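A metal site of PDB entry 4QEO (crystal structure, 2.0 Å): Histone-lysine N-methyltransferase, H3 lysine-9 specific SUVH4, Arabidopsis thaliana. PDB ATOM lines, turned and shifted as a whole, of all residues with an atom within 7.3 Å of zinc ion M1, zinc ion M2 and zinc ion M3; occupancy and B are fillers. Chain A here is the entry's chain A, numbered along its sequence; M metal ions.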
ATOM      1  N   THR A 290      22.972  11.157   8.567  1.00  0.00           N
ATOM      2  CA  THR A 290      21.529  11.375   8.513  1.00  0.00           C
ATOM      3  C   THR A 290      21.174  12.786   8.972  1.00  0.00           C
ATOM      4  O   THR A 290      20.334  13.452   8.370  1.00  0.00           O
ATOM      5  CB  THR A 290      20.778  10.355   9.386  1.00  0.00           C
ATOM      6  OG1 THR A 290      20.932   9.055   8.819  1.00  0.00           O
ATOM      7  CG2 THR A 290      19.295  10.709   9.450  1.00  0.00           C
ATOM      8  N   GLY A 291      21.796  13.230  10.046  1.00  0.00           N
ATOM      9  CA  GLY A 291      21.575  14.570  10.542  1.00  0.00           C
ATOM     10  C   GLY A 291      20.382  14.689  11.469  1.00  0.00           C
ATOM     11  O   GLY A 291      19.685  13.710  11.725  1.00  0.00           O
ATOM     12  N   CYS A 292      20.161  15.906  11.973  1.00  0.00           N
ATOM     13  CA  CYS A 292      19.113  16.173  12.947  1.00  0.00           C
ATOM     14  C   CYS A 292      17.894  16.826  12.307  1.00  0.00           C
ATOM     15  O   CYS A 292      17.962  17.286  11.158  1.00  0.00           O
ATOM     16  CB  CYS A 292      19.678  17.085  14.057  1.00  0.00           C
ATOM     17  SG  CYS A 292      20.111  18.785  13.520  1.00  0.00           S
ATOM     18  N   ASN A 293      16.792  16.902  13.041  1.00  0.00           N
ATOM     19  CA  ASN A 293      15.547  17.416  12.474  1.00  0.00           C
ATOM     20  C   ASN A 293      15.135  18.782  13.017  1.00  0.00           C
ATOM     21  O   ASN A 293      13.993  19.201  12.851  1.00  0.00           O
ATOM     22  CB  ASN A 293      14.396  16.421  12.647  1.00  0.00           C
ATOM     23  CG  ASN A 293      14.004  16.238  14.101  1.00  0.00           C
ATOM     24  OD1 ASN A 293      13.379  17.107  14.703  1.00  0.00           O
ATOM     25  ND2 ASN A 293      14.365  15.096  14.662  1.00  0.00           N
ATOM     26  N   CYS A 294      16.065  19.476  13.666  1.00  0.00           N
ATOM     27  CA  CYS A 294      15.763  20.778  14.260  1.00  0.00           C
ATOM     28  C   CYS A 294      15.443  21.816  13.183  1.00  0.00           C
ATOM     29  O   CYS A 294      15.905  21.702  12.052  1.00  0.00           O
ATOM     30  CB  CYS A 294      16.949  21.242  15.120  1.00  0.00           C
ATOM     31  SG  CYS A 294      17.545  20.009  16.306  1.00  0.00           S
ATOM     32  N   ARG A 295      14.656  22.815  13.534  1.00  0.00           N
ATOM     33  CA  ARG A 295      14.373  23.909  12.618  1.00  0.00           C
ATOM     34  C   ARG A 295      15.126  25.177  13.031  1.00  0.00           C
ATOM     35  O   ARG A 295      15.172  25.523  14.211  1.00  0.00           O
ATOM     36  CB  ARG A 295      12.877  24.208  12.601  1.00  0.00           C
ATOM     37  CG  ARG A 295      12.014  23.114  11.967  1.00  0.00           C
ATOM     38  CD  ARG A 295      10.570  23.259  12.410  1.00  0.00           C
ATOM     39  NE  ARG A 295      10.165  24.661  12.480  1.00  0.00           N
ATOM     40  CZ  ARG A 295       9.153  25.194  11.800  1.00  0.00           C
ATOM     41  NH1 ARG A 295       8.424  24.432  10.996  1.00  0.00           N
ATOM     42  NH2 ARG A 295       8.862  26.476  11.934  1.00  0.00           N
ATOM     43  N   GLY A 296      15.725  25.862  12.056  1.00  0.00           N
ATOM     44  CA  GLY A 296      16.387  27.124  12.315  1.00  0.00           C
ATOM     45  C   GLY A 296      17.764  26.990  12.933  1.00  0.00           C
ATOM     46  O   GLY A 296      18.768  27.115  12.232  1.00  0.00           O
ATOM     47  N   SER A 297      17.814  26.751  14.237  1.00  0.00           N
ATOM     48  CA  SER A 297      19.075  26.517  14.941  1.00  0.00           C
ATOM     49  C   SER A 297      18.932  25.430  15.993  1.00  0.00           C
ATOM     50  O   SER A 297      17.869  25.236  16.560  1.00  0.00           O
ATOM     51  CB  SER A 297      19.579  27.805  15.588  1.00  0.00           C
ATOM     52  OG  SER A 297      19.998  28.736  14.608  1.00  0.00           O
ATOM     53  N   CYS A 298      20.016  24.701  16.248  1.00  0.00           N
ATOM     54  CA  CYS A 298      19.989  23.599  17.203  1.00  0.00           C
ATOM     55  C   CYS A 298      20.352  24.087  18.605  1.00  0.00           C
ATOM     56  O   CYS A 298      21.472  24.558  18.839  1.00  0.00           O
ATOM     57  CB  CYS A 298      20.935  22.489  16.763  1.00  0.00           C
ATOM     58  SG  CYS A 298      20.591  21.921  15.060  1.00  0.00           S
ATOM     59  N   THR A 299      19.382  23.982  19.520  1.00  0.00           N
ATOM     60  CA  THR A 299      19.502  24.558  20.855  1.00  0.00           C
ATOM     61  C   THR A 299      19.258  23.541  21.970  1.00  0.00           C
ATOM     62  O   THR A 299      19.885  23.594  23.029  1.00  0.00           O
ATOM     63  CB  THR A 299      18.512  25.722  21.032  1.00  0.00           C
ATOM     64  OG1 THR A 299      17.179  25.263  20.732  1.00  0.00           O
ATOM     65  CG2 THR A 299      18.869  26.865  20.102  1.00  0.00           C
ATOM     66  N   ASP A 300      18.348  22.600  21.721  1.00  0.00           N
ATOM     67  CA  ASP A 300      18.022  21.617  22.742  1.00  0.00           C
ATOM     68  C   ASP A 300      18.736  20.298  22.518  1.00  0.00           C
ATOM     69  O   ASP A 300      18.548  19.649  21.481  1.00  0.00           O
ATOM     70  CB  ASP A 300      16.516  21.404  22.814  1.00  0.00           C
ATOM     71  CG  ASP A 300      16.128  20.139  23.538  1.00  0.00           C
ATOM     72  OD1 ASP A 300      16.824  19.734  24.498  1.00  0.00           O
ATOM     73  OD2 ASP A 300      15.095  19.543  23.161  1.00  0.00           O
ATOM     74  N   LYS A 303      16.243  17.017  21.818  1.00  0.00           N
ATOM     75  CA  LYS A 303      15.772  16.784  20.449  1.00  0.00           C
ATOM     76  C   LYS A 303      16.897  16.472  19.464  1.00  0.00           C
ATOM     77  O   LYS A 303      16.848  15.452  18.759  1.00  0.00           O
ATOM     78  CB  LYS A 303      14.958  17.987  19.957  1.00  0.00           C
ATOM     79  CG  LYS A 303      13.618  18.152  20.672  1.00  0.00           C
ATOM     80  CD  LYS A 303      13.013  19.527  20.430  1.00  0.00           C
ATOM     81  CE  LYS A 303      11.985  19.870  21.508  1.00  0.00           C
ATOM     82  NZ  LYS A 303      10.725  19.084  21.407  1.00  0.00           N
ATOM     83  N   CYS A 304      17.906  17.333  19.428  1.00  0.00           N
ATOM     84  CA  CYS A 304      18.963  17.278  18.424  1.00  0.00           C
ATOM     85  C   CYS A 304      19.869  16.043  18.477  1.00  0.00           C
ATOM     86  O   CYS A 304      20.626  15.862  19.430  1.00  0.00           O
ATOM     87  CB  CYS A 304      19.846  18.523  18.502  1.00  0.00           C
ATOM     88  SG  CYS A 304      21.071  18.528  17.173  1.00  0.00           S
ATOM     89  N   ALA A 305      19.811  15.240  17.424  1.00  0.00           N
ATOM     90  CA  ALA A 305      20.642  14.039  17.291  1.00  0.00           C
ATOM     91  C   ALA A 305      22.137  14.351  17.199  1.00  0.00           C
ATOM     92  O   ALA A 305      22.985  13.526  17.555  1.00  0.00           O
ATOM     93  CB  ALA A 305      20.216  13.255  16.064  1.00  0.00           C
ATOM     94  N   CYS A 306      22.482  15.521  16.684  1.00  0.00           N
ATOM     95  CA  CYS A 306      23.885  15.842  16.510  1.00  0.00           C
ATOM     96  C   CYS A 306      24.527  16.070  17.891  1.00  0.00           C
ATOM     97  O   CYS A 306      25.645  15.595  18.183  1.00  0.00           O
ATOM     98  CB  CYS A 306      24.059  17.025  15.533  1.00  0.00           C
ATOM     99  SG  CYS A 306      23.199  16.797  13.878  1.00  0.00           S
ATOM    100  N   ALA A 307      23.777  16.722  18.773  1.00  0.00           N
ATOM    101  CA  ALA A 307      24.193  16.862  20.168  1.00  0.00           C
ATOM    102  C   ALA A 307      24.415  15.486  20.788  1.00  0.00           C
ATOM    103  O   ALA A 307      25.433  15.255  21.457  1.00  0.00           O
ATOM    104  CB  ALA A 307      23.142  17.620  20.955  1.00  0.00           C
ATOM    105  N   PHE A 314      26.185  20.204  23.336  1.00  0.00           N
ATOM    106  CA  PHE A 314      26.795  20.976  22.261  1.00  0.00           C
ATOM    107  C   PHE A 314      28.246  21.344  22.578  1.00  0.00           C
ATOM    108  O   PHE A 314      28.537  21.849  23.668  1.00  0.00           O
ATOM    109  CB  PHE A 314      25.978  22.222  21.949  1.00  0.00           C
ATOM    110  CG  PHE A 314      24.618  21.909  21.401  1.00  0.00           C
ATOM    111  CD1 PHE A 314      24.460  21.553  20.073  1.00  0.00           C
ATOM    112  CD2 PHE A 314      23.500  21.941  22.227  1.00  0.00           C
ATOM    113  CE1 PHE A 314      23.200  21.242  19.572  1.00  0.00           C
ATOM    114  CE2 PHE A 314      22.244  21.639  21.730  1.00  0.00           C
ATOM    115  CZ  PHE A 314      22.094  21.294  20.393  1.00  0.00           C
ATOM    116  N   PHE A 332      31.135  16.623  16.323  1.00  0.00           N
ATOM    117  CA  PHE A 332      30.085  16.250  15.376  1.00  0.00           C
ATOM    118  C   PHE A 332      29.217  17.452  15.057  1.00  0.00           C
ATOM    119  O   PHE A 332      28.347  17.835  15.841  1.00  0.00           O
ATOM    120  CB  PHE A 332      29.218  15.128  15.928  1.00  0.00           C
ATOM    121  CG  PHE A 332      29.906  13.795  16.011  1.00  0.00           C
ATOM    122  CD1 PHE A 332      29.944  12.952  14.915  1.00  0.00           C
ATOM    123  CD2 PHE A 332      30.492  13.370  17.194  1.00  0.00           C
ATOM    124  CE1 PHE A 332      30.562  11.707  14.984  1.00  0.00           C
ATOM    125  CE2 PHE A 332      31.108  12.131  17.280  1.00  0.00           C
ATOM    126  CZ  PHE A 332      31.144  11.306  16.172  1.00  0.00           C
ATOM    127  N   GLU A 333      29.463  18.046  13.894  1.00  0.00           N
ATOM    128  CA  GLU A 333      28.712  19.201  13.470  1.00  0.00           C
ATOM    129  C   GLU A 333      27.492  18.814  12.662  1.00  0.00           C
ATOM    130  O   GLU A 333      27.429  17.731  12.062  1.00  0.00           O
ATOM    131  CB  GLU A 333      29.596  20.138  12.638  1.00  0.00           C
ATOM    132  CG  GLU A 333      30.504  21.039  13.469  1.00  0.00           C
ATOM    133  CD  GLU A 333      31.280  22.051  12.643  1.00  0.00           C
ATOM    134  OE1 GLU A 333      31.136  22.060  11.394  1.00  0.00           O
ATOM    135  OE2 GLU A 333      32.033  22.833  13.236  1.00  0.00           O
ATOM    136  N   CYS A 334      26.519  19.717  12.650  1.00  0.00           N
ATOM    137  CA  CYS A 334      25.392  19.614  11.746  1.00  0.00           C
ATOM    138  C   CYS A 334      25.889  19.623  10.300  1.00  0.00           C
ATOM    139  O   CYS A 334      26.923  20.237   9.980  1.00  0.00           O
ATOM    140  CB  CYS A 334      24.382  20.739  12.007  1.00  0.00           C
ATOM    141  SG  CYS A 334      23.506  20.618  13.619  1.00  0.00           S
ATOM    142  N   GLY A 335      25.174  18.916   9.437  1.00  0.00           N
ATOM    143  CA  GLY A 335      25.609  18.715   8.071  1.00  0.00           C
ATOM    144  C   GLY A 335      24.546  18.993   7.020  1.00  0.00           C
ATOM    145  O   GLY A 335      23.534  19.624   7.316  1.00  0.00           O
ATOM    146  N   HIS A 337      22.210  17.297   5.535  1.00  0.00           N
ATOM    147  CA  HIS A 337      20.841  16.837   5.743  1.00  0.00           C
ATOM    148  C   HIS A 337      20.164  17.341   7.016  1.00  0.00           C
ATOM    149  O   HIS A 337      19.001  17.001   7.265  1.00  0.00           O
ATOM    150  CB  HIS A 337      20.759  15.295   5.663  1.00  0.00           C
ATOM    151  CG  HIS A 337      20.995  14.762   4.293  1.00  0.00           C
ATOM    152  ND1 HIS A 337      22.127  14.058   3.949  1.00  0.00           N
ATOM    153  CD2 HIS A 337      20.265  14.868   3.153  1.00  0.00           C
ATOM    154  CE1 HIS A 337      22.076  13.734   2.671  1.00  0.00           C
ATOM    155  NE2 HIS A 337      20.957  14.217   2.170  1.00  0.00           N
ATOM    156  N   CYS A 338      20.860  18.124   7.835  1.00  0.00           N
ATOM    157  CA  CYS A 338      20.235  18.669   9.038  1.00  0.00           C
ATOM    158  C   CYS A 338      19.203  19.732   8.674  1.00  0.00           C
ATOM    159  O   CYS A 338      19.374  20.462   7.694  1.00  0.00           O
ATOM    160  CB  CYS A 338      21.270  19.253  10.014  1.00  0.00           C
ATOM    161  SG  CYS A 338      22.380  18.002  10.691  1.00  0.00           S
ATOM    162  N   GLY A 339      18.145  19.828   9.477  1.00  0.00           N
ATOM    163  CA  GLY A 339      17.056  20.736   9.201  1.00  0.00           C
ATOM    164  C   GLY A 339      17.400  22.180   9.510  1.00  0.00           C
ATOM    165  O   GLY A 339      16.673  23.087   9.105  1.00  0.00           O
ATOM    166  N   CYS A 340      18.499  22.394  10.219  1.00  0.00           N
ATOM    167  CA  CYS A 340      18.920  23.714  10.669  1.00  0.00           C
ATOM    168  C   CYS A 340      19.574  24.498   9.544  1.00  0.00           C
ATOM    169  O   CYS A 340      20.182  23.918   8.631  1.00  0.00           O
ATOM    170  CB  CYS A 340      19.910  23.570  11.825  1.00  0.00           C
ATOM    171  SG  CYS A 340      21.381  22.613  11.375  1.00  0.00           S
ATOM    172  N   GLY A 341      19.460  25.813   9.624  1.00  0.00           N
ATOM    173  CA  GLY A 341      20.102  26.705   8.676  1.00  0.00           C
ATOM    174  C   GLY A 341      21.547  26.984   9.039  1.00  0.00           C
ATOM    175  O   GLY A 341      22.045  26.510  10.052  1.00  0.00           O
ATOM    176  N   LYS A 343      23.146  29.332  10.249  1.00  0.00           N
ATOM    177  CA  LYS A 343      23.466  30.084  11.449  1.00  0.00           C
ATOM    178  C   LYS A 343      23.615  29.194  12.681  1.00  0.00           C
ATOM    179  O   LYS A 343      24.009  29.661  13.740  1.00  0.00           O
ATOM    180  CB  LYS A 343      22.384  31.147  11.713  1.00  0.00           C
ATOM    181  CG  LYS A 343      22.465  32.370  10.802  1.00  0.00           C
ATOM    182  CD  LYS A 343      21.395  33.402  11.180  1.00  0.00           C
ATOM    183  CE  LYS A 343      21.355  34.581  10.203  1.00  0.00           C
ATOM    184  NZ  LYS A 343      20.135  35.454  10.428  1.00  0.00           N
ATOM    185  N   CYS A 344      23.276  27.914  12.539  1.00  0.00           N
ATOM    186  CA  CYS A 344      23.329  26.973  13.666  1.00  0.00           C
ATOM    187  C   CYS A 344      24.688  27.009  14.326  1.00  0.00           C
ATOM    188  O   CYS A 344      25.723  27.000  13.652  1.00  0.00           O
ATOM    189  CB  CYS A 344      23.006  25.540  13.227  1.00  0.00           C
ATOM    190  SG  CYS A 344      23.132  24.341  14.586  1.00  0.00           S
ATOM    191  N   VAL A 345      24.713  27.047  15.656  1.00  0.00           N
ATOM    192  CA  VAL A 345      25.996  27.147  16.364  1.00  0.00           C
ATOM    193  C   VAL A 345      26.778  25.838  16.233  1.00  0.00           C
ATOM    194  O   VAL A 345      28.016  25.815  16.261  1.00  0.00           O
ATOM    195  CB  VAL A 345      25.795  27.582  17.834  1.00  0.00           C
ATOM    196  CG1 VAL A 345      27.137  27.815  18.528  1.00  0.00           C
ATOM    197  CG2 VAL A 345      24.978  28.851  17.879  1.00  0.00           C
ATOM    198  N   ASN A 346      26.038  24.755  16.010  1.00  0.00           N
ATOM    199  CA  ASN A 346      26.686  23.481  15.756  1.00  0.00           C
ATOM    200  C   ASN A 346      27.198  23.335  14.316  1.00  0.00           C
ATOM    201  O   ASN A 346      27.558  22.249  13.876  1.00  0.00           O
ATOM    202  CB  ASN A 346      25.819  22.287  16.173  1.00  0.00           C
ATOM    203  CG  ASN A 346      26.643  21.063  16.508  1.00  0.00           C
ATOM    204  OD1 ASN A 346      27.669  21.159  17.159  1.00  0.00           O
ATOM    205  ND2 ASN A 346      26.215  19.908  16.017  1.00  0.00           N
ATOM    206  N   ARG A 347      27.225  24.447  13.583  1.00  0.00           N
ATOM    207  CA  ARG A 347      27.967  24.529  12.346  1.00  0.00           C
ATOM    208  C   ARG A 347      29.136  25.515  12.475  1.00  0.00           C
ATOM    209  O   ARG A 347      29.599  26.055  11.464  1.00  0.00           O
ATOM    210  CB  ARG A 347      27.044  24.984  11.199  1.00  0.00           C
ATOM    211  CG  ARG A 347      25.840  24.058  10.946  1.00  0.00           C
ATOM    212  CD  ARG A 347      24.963  24.637   9.847  1.00  0.00           C
ATOM    213  NE  ARG A 347      23.819  23.792   9.481  1.00  0.00           N
ATOM    214  CZ  ARG A 347      23.861  22.833   8.563  1.00  0.00           C
ATOM    215  NH1 ARG A 347      25.003  22.558   7.937  1.00  0.00           N
ATOM    216  NH2 ARG A 347      22.767  22.138   8.261  1.00  0.00           N
HETATM  217 ZN    ZN M   1      22.318  18.533  13.012  1.00  0.00          ZN
HETATM  218 ZN    ZN M   2      22.154  22.390  13.635  1.00  0.00          ZN
HETATM  219 ZN    ZN M   3      19.835  19.735  15.647  1.00  0.00          ZN
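N of Cys 306 sits close to SG of Cys 304 (3.4 Å). The backbone carbonyl oxygen (O) of Asn 346 is in hydrogen-bond range of the backbone NH (N) of Cys 334. The backbone NH (N) of Gly 339 sits at hydrogen-bond distance from the backbone carbonyl oxygen (O) of Cys 292, at 3.1 Å. The side-chain sulfur (SG) of Cys 304 sits close to the backbone NH (N) of Ala 307 (3.6 Å). SG of Cys 344 sits close to N of Asn 346 (3.3 Å). The side-chain sulfur (SG) of Cys 338 sits close to the backbone NH (N) of Gly 335 (3.2 Å). The backbone carbonyl oxygen of Cys 294 lies within hydrogen-bond range of the backbone NH of Cys 340 (3.3 Å). The guanidinium group (NH2) of Arg 347 lies within hydrogen-bond range of the backbone carbonyl oxygen (O) of Cys 340 (3.2 Å).
Within 4 Å of zinc ion M2: Cys 298, Cys 334, Cys 340 and Cys 344. Along chain A the residues within 4 Å of zinc ion M2 span positions 298 to 344.
Zinc ion M2 is bound by SG of Cys 298 (2.2 Å), SG of Cys 334 (2.2 Å), SG of Cys 344 (2.4 Å) and SG of Cys 340 (2.4 Å). Zinc ion M2 has four donor atoms within binding distance.
Zinc ion M1 is bound by SG of Cys 306, 2.1 Å away. Zinc ion M1 is bound by SG of Cys 292. SG of Cys 338 binds zinc ion M1, 2.4 Å away. SG of Cys 334 is bound to zinc ion M1, at 2.5 Å. Zinc ion M1 has four donor atoms within binding distance.
Zinc ion M3 is bound by SG of Cys 304 (2.3 Å), SG of Cys 292 (2.3 Å), SG of Cys 298 (2.4 Å) and SG of Cys 294 (2.4 Å). Zinc ion M3 has four donor atoms within binding distance.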
